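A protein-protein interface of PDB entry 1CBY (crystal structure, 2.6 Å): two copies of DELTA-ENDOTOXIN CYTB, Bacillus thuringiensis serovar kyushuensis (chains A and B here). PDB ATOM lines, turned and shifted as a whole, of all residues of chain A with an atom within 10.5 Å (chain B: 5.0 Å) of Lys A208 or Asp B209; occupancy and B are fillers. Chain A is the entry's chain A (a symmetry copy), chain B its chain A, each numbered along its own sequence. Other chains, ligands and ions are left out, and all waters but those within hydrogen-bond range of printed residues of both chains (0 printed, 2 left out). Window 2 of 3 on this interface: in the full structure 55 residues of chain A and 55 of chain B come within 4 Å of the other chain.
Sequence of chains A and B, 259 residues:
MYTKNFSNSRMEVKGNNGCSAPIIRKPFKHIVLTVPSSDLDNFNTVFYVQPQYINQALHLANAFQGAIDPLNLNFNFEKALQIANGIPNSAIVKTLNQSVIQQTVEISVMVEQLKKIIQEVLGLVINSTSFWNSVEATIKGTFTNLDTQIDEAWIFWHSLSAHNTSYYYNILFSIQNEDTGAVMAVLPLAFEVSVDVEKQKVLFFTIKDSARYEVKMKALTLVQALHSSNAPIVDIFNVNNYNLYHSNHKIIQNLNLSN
Lys A208 touches just these residues of chain B: Phe B204, Thr B206 and Asp B209.
Asp B209 touches just one residue of chain A: Lys A208.
No residue of chain A comes within 4 Å of Ile B107.
No residue of chain A comes within 4 Å of Phe B205.
Printed residues of chain B within 4 Å of Phe A204: Lys B208.
Printed residues of chain B within 4 Å of Thr A206: Thr B206 (3.8 Å) and Lys B208 (3.7 Å).
Of the printed residues of chain B, Asp A209 touches Lys B208.
Of the printed residues of chain A, Lys B208 touches Phe A204 (3.4 Å), Thr A206 (3.7 Å) and Asp A209 (3.3 Å).
Ser A210 touches none of the printed residues of chain B.
The nearest printed residue of chain B that does not touch Lys A208 is Phe B205 (5.2 Å).
The nearest residue of chain A that does not touch Asp B209 is Thr A206 (6.8 Å).
The nearest printed residue of chain B that does not touch Thr A206 is Ile B207 (4.4 Å).
The side-chain carboxylate of Asp A209 lies within salt-bridge range of the side-chain amino group of Lys B208, at 3.3 Å.
The side-chain carboxylate (OD2) of Asp B209 lies within salt-bridge range of the side-chain amino group (NZ) of Lys A208, 3.3 Å away.
Of the 11 printed residues of chain B, 4 touch a printed residue of chain A.
Printed residues of chain B that touch a printed residue of chain A: Phe B204, Thr B206, Lys B208 and Asp B209.
Among the printed residues, 7 pairs touch across the chains.
Among the printed residues, Asp or Glu carboxylates within 4 Å of a Lys or Arg side-chain nitrogen of the other chain: Lys A208 with Asp B209 (3.3 Å) and Asp A209 with Lys B208 (3.3 Å).
Phe A204 touches Lys B208, and with the chains exchanged Lys A208 touches Phe B204.
Thr B206 touches its own counterpart, Thr A206.
Thr A206 touches Lys B208, and with the chains exchanged Lys A208 touches Thr B206.
Lys A208 touches Asp B209, and with the chains exchanged Asp A209 touches Lys B208.
The backbone NH (N) of Ile A107 is in hydrogen-bond range of the backbone carbonyl oxygen (O) of Asp A209, at 2.8 Å.
The backbone carbonyl oxygen (O) of Asp B209 is in hydrogen-bond range of the backbone NH (N) of Ile B107, at 2.8 Å.
The backbone NH of Thr B206 lies within hydrogen-bond range of the side-chain carboxylate of Asp B209.
The side-chain carboxylate of Asp A209 lies within hydrogen-bond range of the backbone NH of Thr A206, 2.8 Å away.
Lys B208 touches Phe A204.
Thr B206 touches Thr A206 (CB to CB, 3.8 Å).
CE of Lys B208 touches CG2 of Thr A206, 3.7 Å away.
CE of Lys A208 touches O of Phe B204 (3.4 Å).
Lys A208 touches Thr B206.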
ATOM      1  N   THR A 104      28.534 -11.287  14.458  1.00  0.00           N
ATOM      2  CA  THR A 104      28.305 -10.406  13.325  1.00  0.00           C
ATOM      3  C   THR A 104      29.461 -10.778  12.392  1.00  0.00           C
ATOM      4  O   THR A 104      30.605 -10.875  12.839  1.00  0.00           O
ATOM      5  CB  THR A 104      28.397  -8.913  13.731  1.00  0.00           C
ATOM      6  OG1 THR A 104      27.422  -8.630  14.743  1.00  0.00           O
ATOM      7  CG2 THR A 104      28.136  -8.007  12.533  1.00  0.00           C
ATOM      8  N   VAL A 105      29.152 -11.092  11.141  1.00  0.00           N
ATOM      9  CA  VAL A 105      30.175 -11.465  10.175  1.00  0.00           C
ATOM     10  C   VAL A 105      29.836 -11.050   8.768  1.00  0.00           C
ATOM     11  O   VAL A 105      28.675 -10.802   8.433  1.00  0.00           O
ATOM     12  CB  VAL A 105      30.410 -12.990  10.109  1.00  0.00           C
ATOM     13  CG1 VAL A 105      31.663 -13.361  10.848  1.00  0.00           C
ATOM     14  CG2 VAL A 105      29.214 -13.752  10.635  1.00  0.00           C
ATOM     15  N   GLU A 106      30.881 -10.969   7.955  1.00  0.00           N
ATOM     16  CA  GLU A 106      30.767 -10.645   6.545  1.00  0.00           C
ATOM     17  C   GLU A 106      30.558 -12.019   5.920  1.00  0.00           C
ATOM     18  O   GLU A 106      31.298 -12.958   6.233  1.00  0.00           O
ATOM     19  CB  GLU A 106      32.073 -10.027   6.041  1.00  0.00           C
ATOM     20  CG  GLU A 106      32.031  -9.573   4.592  1.00  0.00           C
ATOM     21  CD  GLU A 106      33.321  -8.911   4.145  1.00  0.00           C
ATOM     22  OE1 GLU A 106      34.018  -8.316   4.996  1.00  0.00           O
ATOM     23  OE2 GLU A 106      33.636  -8.980   2.939  1.00  0.00           O
ATOM     24  N   ILE A 107      29.547 -12.152   5.071  1.00  0.00           N
ATOM     25  CA  ILE A 107      29.239 -13.431   4.443  1.00  0.00           C
ATOM     26  C   ILE A 107      30.458 -14.108   3.818  1.00  0.00           C
ATOM     27  O   ILE A 107      30.619 -15.325   3.940  1.00  0.00           O
ATOM     28  CB  ILE A 107      28.085 -13.300   3.420  1.00  0.00           C
ATOM     29  CG1 ILE A 107      26.824 -12.791   4.136  1.00  0.00           C
ATOM     30  CG2 ILE A 107      27.801 -14.647   2.755  1.00  0.00           C
ATOM     31  CD1 ILE A 107      25.672 -12.466   3.217  1.00  0.00           C
ATOM     32  N   SER A 108      31.339 -13.326   3.199  1.00  0.00           N
ATOM     33  CA  SER A 108      32.540 -13.892   2.585  1.00  0.00           C
ATOM     34  C   SER A 108      33.320 -14.733   3.596  1.00  0.00           C
ATOM     35  O   SER A 108      33.589 -15.913   3.366  1.00  0.00           O
ATOM     36  CB  SER A 108      33.441 -12.781   2.042  1.00  0.00           C
ATOM     37  OG  SER A 108      33.808 -11.879   3.072  1.00  0.00           O
ATOM     38  N   VAL A 109      33.618 -14.136   4.741  1.00  0.00           N
ATOM     39  CA  VAL A 109      34.372 -14.816   5.783  1.00  0.00           C
ATOM     40  C   VAL A 109      33.662 -16.061   6.290  1.00  0.00           C
ATOM     41  O   VAL A 109      34.300 -17.093   6.529  1.00  0.00           O
ATOM     42  CB  VAL A 109      34.651 -13.881   6.979  1.00  0.00           C
ATOM     43  CG1 VAL A 109      35.617 -14.548   7.942  1.00  0.00           C
ATOM     44  CG2 VAL A 109      35.214 -12.552   6.493  1.00  0.00           C
ATOM     45  N   MET A 110      32.343 -15.974   6.439  1.00  0.00           N
ATOM     46  CA  MET A 110      31.545 -17.099   6.933  1.00  0.00           C
ATOM     47  C   MET A 110      31.609 -18.313   6.017  1.00  0.00           C
ATOM     48  O   MET A 110      31.715 -19.445   6.488  1.00  0.00           O
ATOM     49  CB  MET A 110      30.092 -16.671   7.154  1.00  0.00           C
ATOM     50  CG  MET A 110      29.178 -17.783   7.641  1.00  0.00           C
ATOM     51  SD  MET A 110      27.640 -17.136   8.318  1.00  0.00           S
ATOM     52  CE  MET A 110      27.003 -16.244   6.922  1.00  0.00           C
ATOM     53  N   VAL A 111      31.575 -18.080   4.710  1.00  0.00           N
ATOM     54  CA  VAL A 111      31.636 -19.173   3.745  1.00  0.00           C
ATOM     55  C   VAL A 111      32.914 -20.001   3.922  1.00  0.00           C
ATOM     56  O   VAL A 111      32.892 -21.232   3.803  1.00  0.00           O
ATOM     57  CB  VAL A 111      31.550 -18.635   2.302  1.00  0.00           C
ATOM     58  CG1 VAL A 111      31.748 -19.757   1.297  1.00  0.00           C
ATOM     59  CG2 VAL A 111      30.207 -17.978   2.085  1.00  0.00           C
ATOM     60  N   LYS A 140      27.882 -20.410  -0.620  1.00  0.00           N
ATOM     61  CA  LYS A 140      27.568 -19.010  -0.878  1.00  0.00           C
ATOM     62  C   LYS A 140      26.072 -18.861  -1.163  1.00  0.00           C
ATOM     63  O   LYS A 140      25.433 -17.912  -0.704  1.00  0.00           O
ATOM     64  CB  LYS A 140      28.359 -18.490  -2.083  1.00  0.00           C
ATOM     65  CG  LYS A 140      29.846 -18.312  -1.862  1.00  0.00           C
ATOM     66  CD  LYS A 140      30.484 -17.742  -3.120  1.00  0.00           C
ATOM     67  CE  LYS A 140      31.965 -17.469  -2.951  1.00  0.00           C
ATOM     68  NZ  LYS A 140      32.543 -16.947  -4.220  1.00  0.00           N
ATOM     69  N   PHE A 143      23.472 -18.275   1.579  1.00  0.00           N
ATOM     70  CA  PHE A 143      23.323 -16.967   2.208  1.00  0.00           C
ATOM     71  C   PHE A 143      23.088 -15.816   1.236  1.00  0.00           C
ATOM     72  O   PHE A 143      22.634 -14.751   1.647  1.00  0.00           O
ATOM     73  CB  PHE A 143      24.547 -16.651   3.080  1.00  0.00           C
ATOM     74  CG  PHE A 143      24.844 -17.703   4.116  1.00  0.00           C
ATOM     75  CD1 PHE A 143      24.199 -17.692   5.350  1.00  0.00           C
ATOM     76  CD2 PHE A 143      25.749 -18.723   3.848  1.00  0.00           C
ATOM     77  CE1 PHE A 143      24.448 -18.682   6.295  1.00  0.00           C
ATOM     78  CE2 PHE A 143      26.003 -19.715   4.786  1.00  0.00           C
ATOM     79  CZ  PHE A 143      25.348 -19.695   6.013  1.00  0.00           C
ATOM     80  N   THR A 144      23.417 -16.018  -0.037  1.00  0.00           N
ATOM     81  CA  THR A 144      23.253 -14.974  -1.048  1.00  0.00           C
ATOM     82  C   THR A 144      22.378 -15.442  -2.206  1.00  0.00           C
ATOM     83  O   THR A 144      22.185 -16.644  -2.415  1.00  0.00           O
ATOM     84  CB  THR A 144      24.633 -14.473  -1.618  1.00  0.00           C
ATOM     85  OG1 THR A 144      25.408 -15.583  -2.098  1.00  0.00           O
ATOM     86  CG2 THR A 144      25.429 -13.727  -0.553  1.00  0.00           C
ATOM     87  N   ASN A 145      21.849 -14.478  -2.952  1.00  0.00           N
ATOM     88  CA  ASN A 145      20.989 -14.755  -4.093  1.00  0.00           C
ATOM     89  C   ASN A 145      19.754 -15.551  -3.709  1.00  0.00           C
ATOM     90  O   ASN A 145      19.231 -16.328  -4.508  1.00  0.00           O
ATOM     91  CB  ASN A 145      21.764 -15.468  -5.203  1.00  0.00           C
ATOM     92  CG  ASN A 145      22.728 -14.548  -5.917  1.00  0.00           C
ATOM     93  OD1 ASN A 145      22.471 -13.351  -6.069  1.00  0.00           O
ATOM     94  ND2 ASN A 145      23.848 -15.099  -6.364  1.00  0.00           N
ATOM     95  N   PHE A 204      18.493  -9.663  -0.898  1.00  0.00           N
ATOM     96  CA  PHE A 204      19.456  -9.013  -1.777  1.00  0.00           C
ATOM     97  C   PHE A 204      20.858  -8.875  -1.188  1.00  0.00           C
ATOM     98  O   PHE A 204      21.621  -7.984  -1.559  1.00  0.00           O
ATOM     99  CB  PHE A 204      18.908  -7.671  -2.257  1.00  0.00           C
ATOM    100  CG  PHE A 204      17.675  -7.806  -3.099  1.00  0.00           C
ATOM    101  CD1 PHE A 204      17.777  -8.044  -4.465  1.00  0.00           C
ATOM    102  CD2 PHE A 204      16.411  -7.760  -2.518  1.00  0.00           C
ATOM    103  CE1 PHE A 204      16.640  -8.245  -5.241  1.00  0.00           C
ATOM    104  CE2 PHE A 204      15.269  -7.959  -3.284  1.00  0.00           C
ATOM    105  CZ  PHE A 204      15.383  -8.202  -4.649  1.00  0.00           C
ATOM    106  N   PHE A 205      21.191  -9.795  -0.289  1.00  0.00           N
ATOM    107  CA  PHE A 205      22.498  -9.841   0.345  1.00  0.00           C
ATOM    108  C   PHE A 205      23.574 -10.311  -0.639  1.00  0.00           C
ATOM    109  O   PHE A 205      23.334 -11.179  -1.483  1.00  0.00           O
ATOM    110  CB  PHE A 205      22.458 -10.807   1.526  1.00  0.00           C
ATOM    111  CG  PHE A 205      22.197 -10.149   2.843  1.00  0.00           C
ATOM    112  CD1 PHE A 205      21.959  -8.778   2.921  1.00  0.00           C
ATOM    113  CD2 PHE A 205      22.229 -10.898   4.017  1.00  0.00           C
ATOM    114  CE1 PHE A 205      21.756  -8.160   4.156  1.00  0.00           C
ATOM    115  CE2 PHE A 205      22.029 -10.292   5.252  1.00  0.00           C
ATOM    116  CZ  PHE A 205      21.794  -8.918   5.323  1.00  0.00           C
ATOM    117  N   THR A 206      24.769  -9.752  -0.510  1.00  0.00           N
ATOM    118  CA  THR A 206      25.891 -10.120  -1.363  1.00  0.00           C
ATOM    119  C   THR A 206      27.028 -10.660  -0.487  1.00  0.00           C
ATOM    120  O   THR A 206      26.986 -10.544   0.738  1.00  0.00           O
ATOM    121  CB  THR A 206      26.397  -8.911  -2.183  1.00  0.00           C
ATOM    122  OG1 THR A 206      26.844  -7.880  -1.297  1.00  0.00           O
ATOM    123  CG2 THR A 206      25.291  -8.365  -3.070  1.00  0.00           C
ATOM    124  N   ILE A 207      28.031 -11.261  -1.118  1.00  0.00           N
ATOM    125  CA  ILE A 207      29.188 -11.823  -0.421  1.00  0.00           C
ATOM    126  C   ILE A 207      29.865 -10.812   0.512  1.00  0.00           C
ATOM    127  O   ILE A 207      30.453 -11.186   1.537  1.00  0.00           O
ATOM    128  CB  ILE A 207      30.215 -12.367  -1.456  1.00  0.00           C
ATOM    129  CG1 ILE A 207      29.711 -13.678  -2.062  1.00  0.00           C
ATOM    130  CG2 ILE A 207      31.572 -12.594  -0.827  1.00  0.00           C
ATOM    131  CD1 ILE A 207      29.603 -14.811  -1.062  1.00  0.00           C
ATOM    132  N   LYS A 208      29.733  -9.531   0.179  1.00  0.00           N
ATOM    133  CA  LYS A 208      30.345  -8.456   0.950  1.00  0.00           C
ATOM    134  C   LYS A 208      29.513  -7.921   2.116  1.00  0.00           C
ATOM    135  O   LYS A 208      29.941  -6.995   2.807  1.00  0.00           O
ATOM    136  CB  LYS A 208      30.676  -7.288   0.022  1.00  0.00           C
ATOM    137  CG  LYS A 208      31.485  -7.654  -1.212  1.00  0.00           C
ATOM    138  CD  LYS A 208      31.728  -6.413  -2.060  1.00  0.00           C
ATOM    139  CE  LYS A 208      32.536  -6.718  -3.305  1.00  0.00           C
ATOM    140  NZ  LYS A 208      32.838  -5.471  -4.065  1.00  0.00           N
ATOM    141  N   ASP A 209      28.324  -8.471   2.328  1.00  0.00           N
ATOM    142  CA  ASP A 209      27.472  -7.985   3.406  1.00  0.00           C
ATOM    143  C   ASP A 209      27.739  -8.592   4.764  1.00  0.00           C
ATOM    144  O   ASP A 209      28.221  -9.714   4.870  1.00  0.00           O
ATOM    145  CB  ASP A 209      25.997  -8.104   3.030  1.00  0.00           C
ATOM    146  CG  ASP A 209      25.567  -7.025   2.052  1.00  0.00           C
ATOM    147  OD1 ASP A 209      25.724  -5.828   2.375  1.00  0.00           O
ATOM    148  OD2 ASP A 209      25.091  -7.365   0.953  1.00  0.00           O
ATOM    149  N   SER A 210      27.430  -7.827   5.803  1.00  0.00           N
ATOM    150  CA  SER A 210      27.634  -8.260   7.174  1.00  0.00           C
ATOM    151  C   SER A 210      26.310  -8.251   7.931  1.00  0.00           C
ATOM    152  O   SER A 210      25.389  -7.508   7.581  1.00  0.00           O
ATOM    153  CB  SER A 210      28.620  -7.319   7.873  1.00  0.00           C
ATOM    154  OG  SER A 210      29.797  -7.139   7.105  1.00  0.00           O
ATOM    155  N   ALA A 211      26.222  -9.069   8.973  1.00  0.00           N
ATOM    156  CA  ALA A 211      25.023  -9.149   9.797  1.00  0.00           C
ATOM    157  C   ALA A 211      25.293 -10.106  10.945  1.00  0.00           C
ATOM    158  O   ALA A 211      26.204 -10.934  10.868  1.00  0.00           O
ATOM    159  CB  ALA A 211      23.835  -9.638   8.969  1.00  0.00           C
ATOM    160  N   TYR A 213      24.841 -13.151  12.689  1.00  0.00           N
ATOM    161  CA  TYR A 213      24.372 -14.463  12.287  1.00  0.00           C
ATOM    162  C   TYR A 213      24.391 -15.516  13.379  1.00  0.00           C
ATOM    163  O   TYR A 213      25.259 -15.524  14.260  1.00  0.00           O
ATOM    164  CB  TYR A 213      25.210 -14.990  11.121  1.00  0.00           C
ATOM    165  CG  TYR A 213      24.733 -14.565   9.758  1.00  0.00           C
ATOM    166  CD1 TYR A 213      23.789 -15.322   9.065  1.00  0.00           C
ATOM    167  CD2 TYR A 213      25.232 -13.419   9.147  1.00  0.00           C
ATOM    168  CE1 TYR A 213      23.354 -14.945   7.798  1.00  0.00           C
ATOM    169  CE2 TYR A 213      24.802 -13.036   7.877  1.00  0.00           C
ATOM    170  CZ  TYR A 213      23.861 -13.804   7.215  1.00  0.00           C
ATOM    171  OH  TYR A 213      23.400 -13.409   5.983  1.00  0.00           O
ATOM    172  N   VAL B 105      27.178   0.151 -16.076  1.00  0.00           N
ATOM    173  CA  VAL B 105      25.962  -0.362 -15.463  1.00  0.00           C
ATOM    174  C   VAL B 105      26.223  -1.139 -14.199  1.00  0.00           C
ATOM    175  O   VAL B 105      27.334  -1.615 -13.954  1.00  0.00           O
ATOM    176  CB  VAL B 105      25.186  -1.328 -16.386  1.00  0.00           C
ATOM    177  CG1 VAL B 105      24.004  -0.634 -16.997  1.00  0.00           C
ATOM    178  CG2 VAL B 105      26.089  -1.915 -17.448  1.00  0.00           C
ATOM    179  N   GLU B 106      25.172  -1.246 -13.395  1.00  0.00           N
ATOM    180  CA  GLU B 106      25.192  -2.003 -12.157  1.00  0.00           C
ATOM    181  C   GLU B 106      24.799  -3.396 -12.633  1.00  0.00           C
ATOM    182  O   GLU B 106      23.824  -3.542 -13.377  1.00  0.00           O
ATOM    183  CB  GLU B 106      24.140  -1.456 -11.192  1.00  0.00           C
ATOM    184  CG  GLU B 106      24.134  -2.127  -9.829  1.00  0.00           C
ATOM    185  CD  GLU B 106      23.120  -1.520  -8.878  1.00  0.00           C
ATOM    186  OE1 GLU B 106      22.814  -0.315  -9.013  1.00  0.00           O
ATOM    187  OE2 GLU B 106      22.632  -2.246  -7.988  1.00  0.00           O
ATOM    188  N   ILE B 107      25.561  -4.409 -12.239  1.00  0.00           N
ATOM    189  CA  ILE B 107      25.293  -5.778 -12.663  1.00  0.00           C
ATOM    190  C   ILE B 107      23.837  -6.196 -12.472  1.00  0.00           C
ATOM    191  O   ILE B 107      23.267  -6.861 -13.342  1.00  0.00           O
ATOM    192  CB  ILE B 107      26.258  -6.782 -11.987  1.00  0.00           C
ATOM    193  CG1 ILE B 107      27.707  -6.429 -12.360  1.00  0.00           C
ATOM    194  CG2 ILE B 107      25.939  -8.211 -12.424  1.00  0.00           C
ATOM    195  CD1 ILE B 107      28.754  -7.236 -11.633  1.00  0.00           C
ATOM    196  N   PHE B 204      35.791 -10.691  -7.776  1.00  0.00           N
ATOM    197  CA  PHE B 204      35.012 -10.493  -6.562  1.00  0.00           C
ATOM    198  C   PHE B 204      33.854  -9.509  -6.704  1.00  0.00           C
ATOM    199  O   PHE B 204      33.419  -8.891  -5.733  1.00  0.00           O
ATOM    200  CB  PHE B 204      35.933 -10.123  -5.400  1.00  0.00           C
ATOM    201  CG  PHE B 204      36.900 -11.212  -5.044  1.00  0.00           C
ATOM    202  CD1 PHE B 204      36.524 -12.233  -4.180  1.00  0.00           C
ATOM    203  CD2 PHE B 204      38.164 -11.255  -5.625  1.00  0.00           C
ATOM    204  CE1 PHE B 204      37.388 -13.287  -3.902  1.00  0.00           C
ATOM    205  CE2 PHE B 204      39.036 -12.302  -5.354  1.00  0.00           C
ATOM    206  CZ  PHE B 204      38.647 -13.322  -4.491  1.00  0.00           C
ATOM    207  N   PHE B 205      33.344  -9.403  -7.926  1.00  0.00           N
ATOM    208  CA  PHE B 205      32.214  -8.543  -8.237  1.00  0.00           C
ATOM    209  C   PHE B 205      30.912  -9.114  -7.666  1.00  0.00           C
ATOM    210  O   PHE B 205      30.699 -10.329  -7.650  1.00  0.00           O
ATOM    211  CB  PHE B 205      32.072  -8.416  -9.752  1.00  0.00           C
ATOM    212  CG  PHE B 205      32.738  -7.208 -10.327  1.00  0.00           C
ATOM    213  CD1 PHE B 205      33.464  -6.337  -9.515  1.00  0.00           C
ATOM    214  CD2 PHE B 205      32.607  -6.916 -11.682  1.00  0.00           C
ATOM    215  CE1 PHE B 205      34.050  -5.189 -10.047  1.00  0.00           C
ATOM    216  CE2 PHE B 205      33.187  -5.773 -12.223  1.00  0.00           C
ATOM    217  CZ  PHE B 205      33.909  -4.906 -11.404  1.00  0.00           C
ATOM    218  N   THR B 206      30.031  -8.229  -7.223  1.00  0.00           N
ATOM    219  CA  THR B 206      28.742  -8.629  -6.674  1.00  0.00           C
ATOM    220  C   THR B 206      27.625  -7.998  -7.515  1.00  0.00           C
ATOM    221  O   THR B 206      27.881  -7.128  -8.348  1.00  0.00           O
ATOM    222  CB  THR B 206      28.594  -8.191  -5.200  1.00  0.00           C
ATOM    223  OG1 THR B 206      28.681  -6.765  -5.110  1.00  0.00           O
ATOM    224  CG2 THR B 206      29.683  -8.814  -4.343  1.00  0.00           C
ATOM    225  N   ILE B 207      26.393  -8.449  -7.300  1.00  0.00           N
ATOM    226  CA  ILE B 207      25.224  -7.942  -8.020  1.00  0.00           C
ATOM    227  C   ILE B 207      25.099  -6.416  -7.944  1.00  0.00           C
ATOM    228  O   ILE B 207      24.568  -5.775  -8.863  1.00  0.00           O
ATOM    229  CB  ILE B 207      23.933  -8.613  -7.468  1.00  0.00           C
ATOM    230  CG1 ILE B 207      23.838 -10.060  -7.957  1.00  0.00           C
ATOM    231  CG2 ILE B 207      22.690  -7.858  -7.887  1.00  0.00           C
ATOM    232  CD1 ILE B 207      23.671 -10.186  -9.458  1.00  0.00           C
ATOM    233  N   LYS B 208      25.635  -5.839  -6.874  1.00  0.00           N
ATOM    234  CA  LYS B 208      25.569  -4.400  -6.646  1.00  0.00           C
ATOM    235  C   LYS B 208      26.695  -3.579  -7.273  1.00  0.00           C
ATOM    236  O   LYS B 208      26.735  -2.358  -7.111  1.00  0.00           O
ATOM    237  CB  LYS B 208      25.552  -4.122  -5.143  1.00  0.00           C
ATOM    238  CG  LYS B 208      24.498  -4.884  -4.358  1.00  0.00           C
ATOM    239  CD  LYS B 208      24.600  -4.538  -2.879  1.00  0.00           C
ATOM    240  CE  LYS B 208      23.567  -5.269  -2.045  1.00  0.00           C
ATOM    241  NZ  LYS B 208      23.630  -4.838  -0.620  1.00  0.00           N
ATOM    242  N   ASP B 209      27.624  -4.230  -7.963  1.00  0.00           N
ATOM    243  CA  ASP B 209      28.738  -3.506  -8.560  1.00  0.00           C
ATOM    244  C   ASP B 209      28.468  -2.915  -9.923  1.00  0.00           C
ATOM    245  O   ASP B 209      27.635  -3.411 -10.672  1.00  0.00           O
ATOM    246  CB  ASP B 209      30.001  -4.365  -8.572  1.00  0.00           C
ATOM    247  CG  ASP B 209      30.646  -4.454  -7.200  1.00  0.00           C
ATOM    248  OD1 ASP B 209      30.979  -3.395  -6.627  1.00  0.00           O
ATOM    249  OD2 ASP B 209      30.805  -5.574  -6.682  1.00  0.00           O
ATOM    250  N   SER B 210      29.178  -1.837 -10.230  1.00  0.00           N
ATOM    251  CA  SER B 210      29.030  -1.145 -11.499  1.00  0.00           C
ATOM    252  C   SER B 210      30.363  -1.117 -12.241  1.00  0.00           C
ATOM    253  O   SER B 210      31.429  -1.190 -11.625  1.00  0.00           O
ATOM    254  CB  SER B 210      28.561   0.292 -11.253  1.00  0.00           C
ATOM    255  OG  SER B 210      27.431   0.329 -10.398  1.00  0.00           O
ATOM    256  N   ALA B 211      30.297  -1.002 -13.562  1.00  0.00           N
ATOM    257  CA  ALA B 211      31.491  -0.944 -14.394  1.00  0.00           C
ATOM    258  C   ALA B 211      31.062  -0.720 -15.834  1.00  0.00           C
ATOM    259  O   ALA B 211      29.913  -0.989 -16.193  1.00  0.00           O
ATOM    260  CB  ALA B 211      32.291  -2.241 -14.277  1.00  0.00           C
